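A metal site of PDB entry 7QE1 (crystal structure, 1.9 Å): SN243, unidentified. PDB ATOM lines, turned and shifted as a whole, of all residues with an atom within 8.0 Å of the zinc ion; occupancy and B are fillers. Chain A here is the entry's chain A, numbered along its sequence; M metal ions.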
ATOM      1  N   GLU A  20      -7.943 -12.606 -10.340  1.00  0.00           N
ATOM      2  CA  GLU A  20      -8.044 -14.074 -10.461  1.00  0.00           C
ATOM      3  C   GLU A  20      -9.487 -14.484 -10.165  1.00  0.00           C
ATOM      4  O   GLU A  20     -10.162 -13.800  -9.395  1.00  0.00           O
ATOM      5  CB  GLU A  20      -7.081 -14.762  -9.499  1.00  0.00           C
ATOM      6  CG  GLU A  20      -5.625 -14.396  -9.726  1.00  0.00           C
ATOM      7  CD  GLU A  20      -4.712 -15.583  -9.984  1.00  0.00           C
ATOM      8  OE1 GLU A  20      -3.770 -15.438 -10.787  1.00  0.00           O
ATOM      9  OE2 GLU A  20      -4.939 -16.645  -9.366  1.00  0.00           O
ATOM     10  N   ILE A  22     -12.220 -16.654  -8.366  1.00  0.00           N
ATOM     11  CA  ILE A  22     -12.302 -17.423  -7.093  1.00  0.00           C
ATOM     12  C   ILE A  22     -13.603 -18.200  -7.126  1.00  0.00           C
ATOM     13  O   ILE A  22     -14.575 -17.696  -7.711  1.00  0.00           O
ATOM     14  CB  ILE A  22     -12.235 -16.458  -5.895  1.00  0.00           C
ATOM     15  CG1 ILE A  22     -10.805 -15.987  -5.615  1.00  0.00           C
ATOM     16  CG2 ILE A  22     -12.871 -17.071  -4.660  1.00  0.00           C
ATOM     17  CD1 ILE A  22     -10.691 -15.138  -4.374  1.00  0.00           C
ATOM     18  N   ARG A  30     -15.057 -13.107  -9.155  1.00  0.00           N
ATOM     19  CA  ARG A  30     -13.772 -12.433  -9.442  1.00  0.00           C
ATOM     20  C   ARG A  30     -13.270 -11.736  -8.176  1.00  0.00           C
ATOM     21  O   ARG A  30     -14.078 -11.086  -7.510  1.00  0.00           O
ATOM     22  CB  ARG A  30     -13.938 -11.405 -10.568  1.00  0.00           C
ATOM     23  CG  ARG A  30     -14.583 -11.939 -11.837  1.00  0.00           C
ATOM     24  CD  ARG A  30     -14.988 -10.809 -12.758  1.00  0.00           C
ATOM     25  NE  ARG A  30     -13.853 -10.165 -13.399  1.00  0.00           N
ATOM     26  CZ  ARG A  30     -13.780  -8.869 -13.689  1.00  0.00           C
ATOM     27  NH1 ARG A  30     -14.788  -8.070 -13.384  1.00  0.00           N
ATOM     28  NH2 ARG A  30     -12.710  -8.386 -14.271  1.00  0.00           N
ATOM     29  N   ASP A  31     -11.985 -11.882  -7.866  1.00  0.00           N
ATOM     30  CA  ASP A  31     -11.414 -11.202  -6.681  1.00  0.00           C
ATOM     31  C   ASP A  31     -10.792  -9.880  -7.136  1.00  0.00           C
ATOM     32  O   ASP A  31      -9.590  -9.863  -7.428  1.00  0.00           O
ATOM     33  CB  ASP A  31     -10.389 -12.053  -5.926  1.00  0.00           C
ATOM     34  CG  ASP A  31     -10.307 -11.666  -4.461  1.00  0.00           C
ATOM     35  OD1 ASP A  31     -11.359 -11.324  -3.891  1.00  0.00           O
ATOM     36  OD2 ASP A  31      -9.200 -11.700  -3.905  1.00  0.00           O
ATOM     37  N   LEU A  32     -11.613  -8.831  -7.176  1.00  0.00           N
ATOM     38  CA  LEU A  32     -11.117  -7.529  -7.696  1.00  0.00           C
ATOM     39  C   LEU A  32     -10.233  -6.859  -6.639  1.00  0.00           C
ATOM     40  O   LEU A  32      -9.437  -5.974  -7.018  1.00  0.00           O
ATOM     41  CB  LEU A  32     -12.335  -6.680  -8.056  1.00  0.00           C
ATOM     42  CG  LEU A  32     -13.323  -7.331  -9.021  1.00  0.00           C
ATOM     43  CD1 LEU A  32     -14.603  -6.521  -9.127  1.00  0.00           C
ATOM     44  CD2 LEU A  32     -12.690  -7.522 -10.390  1.00  0.00           C
ATOM     45  N   ASN A  33     -10.359  -7.273  -5.378  1.00  0.00           N
ATOM     46  CA  ASN A  33      -9.529  -6.693  -4.282  1.00  0.00           C
ATOM     47  C   ASN A  33      -8.256  -7.527  -4.093  1.00  0.00           C
ATOM     48  O   ASN A  33      -7.328  -7.029  -3.440  1.00  0.00           O
ATOM     49  CB  ASN A  33     -10.332  -6.565  -2.978  1.00  0.00           C
ATOM     50  CG  ASN A  33     -10.681  -7.895  -2.351  1.00  0.00           C
ATOM     51  OD1 ASN A  33     -10.647  -8.936  -3.004  1.00  0.00           O
ATOM     52  ND2 ASN A  33     -11.028  -7.866  -1.076  1.00  0.00           N
ATOM     53  N   ASP A  34      -8.221  -8.740  -4.650  1.00  0.00           N
ATOM     54  CA  ASP A  34      -7.014  -9.606  -4.581  1.00  0.00           C
ATOM     55  C   ASP A  34      -6.704  -9.937  -3.124  1.00  0.00           C
ATOM     56  O   ASP A  34      -5.518 -10.091  -2.791  1.00  0.00           O
ATOM     57  CB  ASP A  34      -5.822  -8.941  -5.290  1.00  0.00           C
ATOM     58  CG  ASP A  34      -4.750  -9.931  -5.708  1.00  0.00           C
ATOM     59  OD1 ASP A  34      -4.976 -11.146  -5.548  1.00  0.00           O
ATOM     60  OD2 ASP A  34      -3.688  -9.483  -6.192  1.00  0.00           O
ATOM     61  N   ASN A  35      -7.742 -10.034  -2.281  1.00  0.00           N
ATOM     62  CA  ASN A  35      -7.551 -10.401  -0.863  1.00  0.00           C
ATOM     63  C   ASN A  35      -7.473 -11.931  -0.774  1.00  0.00           C
ATOM     64  O   ASN A  35      -6.891 -12.445   0.194  1.00  0.00           O
ATOM     65  CB  ASN A  35      -8.669  -9.870   0.021  1.00  0.00           C
ATOM     66  CG  ASN A  35     -10.021 -10.444  -0.341  1.00  0.00           C
ATOM     67  OD1 ASN A  35     -10.203 -10.993  -1.424  1.00  0.00           O
ATOM     68  ND2 ASN A  35     -10.987 -10.314   0.555  1.00  0.00           N
ATOM     69  N   GLY A  36      -8.042 -12.620  -1.763  1.00  0.00           N
ATOM     70  CA  GLY A  36      -8.088 -14.096  -1.733  1.00  0.00           C
ATOM     71  C   GLY A  36      -9.409 -14.556  -1.185  1.00  0.00           C
ATOM     72  O   GLY A  36      -9.627 -15.774  -1.089  1.00  0.00           O
ATOM     73  N   GLU A  37     -10.275 -13.606  -0.826  1.00  0.00           N
ATOM     74  CA  GLU A  37     -11.586 -13.952  -0.214  1.00  0.00           C
ATOM     75  C   GLU A  37     -12.705 -13.317  -1.031  1.00  0.00           C
ATOM     76  O   GLU A  37     -12.462 -12.268  -1.657  1.00  0.00           O
ATOM     77  CB  GLU A  37     -11.638 -13.455   1.220  1.00  0.00           C
ATOM     78  CG  GLU A  37     -10.667 -14.177   2.144  1.00  0.00           C
ATOM     79  CD  GLU A  37     -10.628 -13.651   3.573  1.00  0.00           C
ATOM     80  OE1 GLU A  37     -11.235 -12.593   3.827  1.00  0.00           O
ATOM     81  OE2 GLU A  37     -10.002 -14.310   4.422  1.00  0.00           O
ATOM     82  N   LEU A  38     -13.897 -13.922  -1.022  1.00  0.00           N
ATOM     83  CA  LEU A  38     -15.050 -13.343  -1.746  1.00  0.00           C
ATOM     84  C   LEU A  38     -15.644 -12.228  -0.893  1.00  0.00           C
ATOM     85  O   LEU A  38     -16.448 -12.542   0.010  1.00  0.00           O
ATOM     86  CB  LEU A  38     -16.090 -14.427  -2.012  1.00  0.00           C
ATOM     87  CG  LEU A  38     -17.378 -13.941  -2.669  1.00  0.00           C
ATOM     88  CD1 LEU A  38     -17.087 -13.245  -3.989  1.00  0.00           C
ATOM     89  CD2 LEU A  38     -18.354 -15.086  -2.886  1.00  0.00           C
ATOM     90  N   ASP A  39     -15.251 -10.978  -1.148  1.00  0.00           N
ATOM     91  CA  ASP A  39     -15.877  -9.849  -0.425  1.00  0.00           C
ATOM     92  C   ASP A  39     -17.296  -9.672  -0.965  1.00  0.00           C
ATOM     93  O   ASP A  39     -17.500  -9.939  -2.163  1.00  0.00           O
ATOM     94  CB  ASP A  39     -15.015  -8.592  -0.538  1.00  0.00           C
ATOM     95  CG  ASP A  39     -13.533  -8.886  -0.396  1.00  0.00           C
ATOM     96  OD1 ASP A  39     -13.002  -9.645  -1.237  1.00  0.00           O
ATOM     97  OD2 ASP A  39     -12.926  -8.358   0.550  1.00  0.00           O
ATOM     98  N   PRO A  40     -18.277  -9.244  -0.146  1.00  0.00           N
ATOM     99  CA  PRO A  40     -19.667  -9.170  -0.598  1.00  0.00           C
ATOM    100  C   PRO A  40     -19.867  -8.434  -1.938  1.00  0.00           C
ATOM    101  O   PRO A  40     -20.680  -8.875  -2.711  1.00  0.00           O
ATOM    102  CB  PRO A  40     -20.345  -8.400   0.539  1.00  0.00           C
ATOM    103  CG  PRO A  40     -19.530  -8.749   1.757  1.00  0.00           C
ATOM    104  CD  PRO A  40     -18.104  -8.840   1.241  1.00  0.00           C
ATOM    105  N   TYR A  41     -19.128  -7.344  -2.165  1.00  0.00           N
ATOM    106  CA  TYR A  41     -19.350  -6.549  -3.399  1.00  0.00           C
ATOM    107  C   TYR A  41     -18.942  -7.395  -4.609  1.00  0.00           C
ATOM    108  O   TYR A  41     -19.418  -7.114  -5.732  1.00  0.00           O
ATOM    109  CB  TYR A  41     -18.625  -5.198  -3.328  1.00  0.00           C
ATOM    110  CG  TYR A  41     -17.163  -5.218  -3.686  1.00  0.00           C
ATOM    111  CD1 TYR A  41     -16.743  -5.014  -4.989  1.00  0.00           C
ATOM    112  CD2 TYR A  41     -16.193  -5.392  -2.709  1.00  0.00           C
ATOM    113  CE1 TYR A  41     -15.400  -5.014  -5.318  1.00  0.00           C
ATOM    114  CE2 TYR A  41     -14.840  -5.396  -3.028  1.00  0.00           C
ATOM    115  CZ  TYR A  41     -14.450  -5.198  -4.339  1.00  0.00           C
ATOM    116  OH  TYR A  41     -13.119  -5.198  -4.657  1.00  0.00           O
ATOM    117  N   GLU A  42     -18.084  -8.399  -4.392  1.00  0.00           N
ATOM    118  CA  GLU A  42     -17.651  -9.295  -5.499  1.00  0.00           C
ATOM    119  C   GLU A  42     -18.672 -10.420  -5.643  1.00  0.00           C
ATOM    120  O   GLU A  42     -18.461 -11.285  -6.508  1.00  0.00           O
ATOM    121  CB  GLU A  42     -16.282  -9.875  -5.170  1.00  0.00           C
ATOM    122  CG  GLU A  42     -15.249  -8.846  -4.758  1.00  0.00           C
ATOM    123  CD  GLU A  42     -13.937  -9.429  -4.261  1.00  0.00           C
ATOM    124  OE1 GLU A  42     -13.968 -10.509  -3.649  1.00  0.00           O
ATOM    125  OE2 GLU A  42     -12.885  -8.804  -4.508  1.00  0.00           O
ATOM    126  N   ASP A  54     -20.895  -2.585   0.682  1.00  0.00           N
ATOM    127  CA  ASP A  54     -19.631  -3.252   0.997  1.00  0.00           C
ATOM    128  C   ASP A  54     -18.453  -2.613   0.280  1.00  0.00           C
ATOM    129  O   ASP A  54     -17.328  -2.590   0.804  1.00  0.00           O
ATOM    130  CB  ASP A  54     -19.713  -4.751   0.677  1.00  0.00           C
ATOM    131  CG  ASP A  54     -18.395  -5.473   0.955  1.00  0.00           C
ATOM    132  OD1 ASP A  54     -17.998  -5.568   2.135  1.00  0.00           O
ATOM    133  OD2 ASP A  54     -17.760  -5.929  -0.010  1.00  0.00           O
ATOM    134  N   GLN A  58     -15.040   0.101   1.693  1.00  0.00           N
ATOM    135  CA  GLN A  58     -13.645  -0.252   1.504  1.00  0.00           C
ATOM    136  C   GLN A  58     -12.823   0.809   0.770  1.00  0.00           C
ATOM    137  O   GLN A  58     -11.608   0.630   0.631  1.00  0.00           O
ATOM    138  CB  GLN A  58     -13.521  -1.576   0.719  1.00  0.00           C
ATOM    139  CG  GLN A  58     -14.360  -2.722   1.236  1.00  0.00           C
ATOM    140  CD  GLN A  58     -14.150  -3.983   0.433  1.00  0.00           C
ATOM    141  OE1 GLN A  58     -13.082  -4.193  -0.148  1.00  0.00           O
ATOM    142  NE2 GLN A  58     -15.165  -4.842   0.392  1.00  0.00           N
ATOM    143  N   ARG A 146      -6.717  -1.332  -7.296  1.00  0.00           N
ATOM    144  CA  ARG A 146      -6.885  -2.050  -6.019  1.00  0.00           C
ATOM    145  C   ARG A 146      -8.228  -2.754  -5.962  1.00  0.00           C
ATOM    146  O   ARG A 146      -8.241  -3.949  -5.740  1.00  0.00           O
ATOM    147  CB  ARG A 146      -6.759  -1.048  -4.874  1.00  0.00           C
ATOM    148  CG  ARG A 146      -7.129  -1.590  -3.508  1.00  0.00           C
ATOM    149  CD  ARG A 146      -6.582  -0.703  -2.408  1.00  0.00           C
ATOM    150  NE  ARG A 146      -7.549   0.297  -1.996  1.00  0.00           N
ATOM    151  CZ  ARG A 146      -8.598   0.049  -1.220  1.00  0.00           C
ATOM    152  NH1 ARG A 146      -8.816  -1.173  -0.775  1.00  0.00           N
ATOM    153  NH2 ARG A 146      -9.430   1.022  -0.891  1.00  0.00           N
HETATM  154 ZN    ZN M   1     -11.949 -10.230  -2.573  1.00  0.00          ZN
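The zinc ion is bound by the side-chain carboxylate (OD1) of Asp 39, the side-chain carboxylate (OD1) of Asp 31, the side-chain amide oxygen (OD1) of Asn 33, the side-chain amide oxygen (OD1) of Asn 35, the backbone carbonyl oxygen (O) of Glu 37, the side-chain carboxylate (OE1) of Glu 42 and the side-chain carboxylate (OE2) of Glu 42. The zinc ion has seven donor atoms within binding distance.
The side-chain carboxylate (OD2) of Asp 31 sits at hydrogen-bond distance from the backbone NH (N) of Gly 36, 2.6 Å away. The backbone NH (N) of Asp 34 lies close to the side-chain carboxylate (OD2) of Asp 31 (3.2 Å). The backbone NH (N) of Leu 32 lies close to the side-chain carboxylate (OE2) of Glu 42, 3.0 Å away. N of Asp 31 lies within hydrogen-bond range of O of Glu 20 (3.1 Å).
Of the 18 residues printed, 6 come within 4 Å of the zinc ion. The nearest printed residue that does not touch the zinc ion is Leu 38 (4.5 Å).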
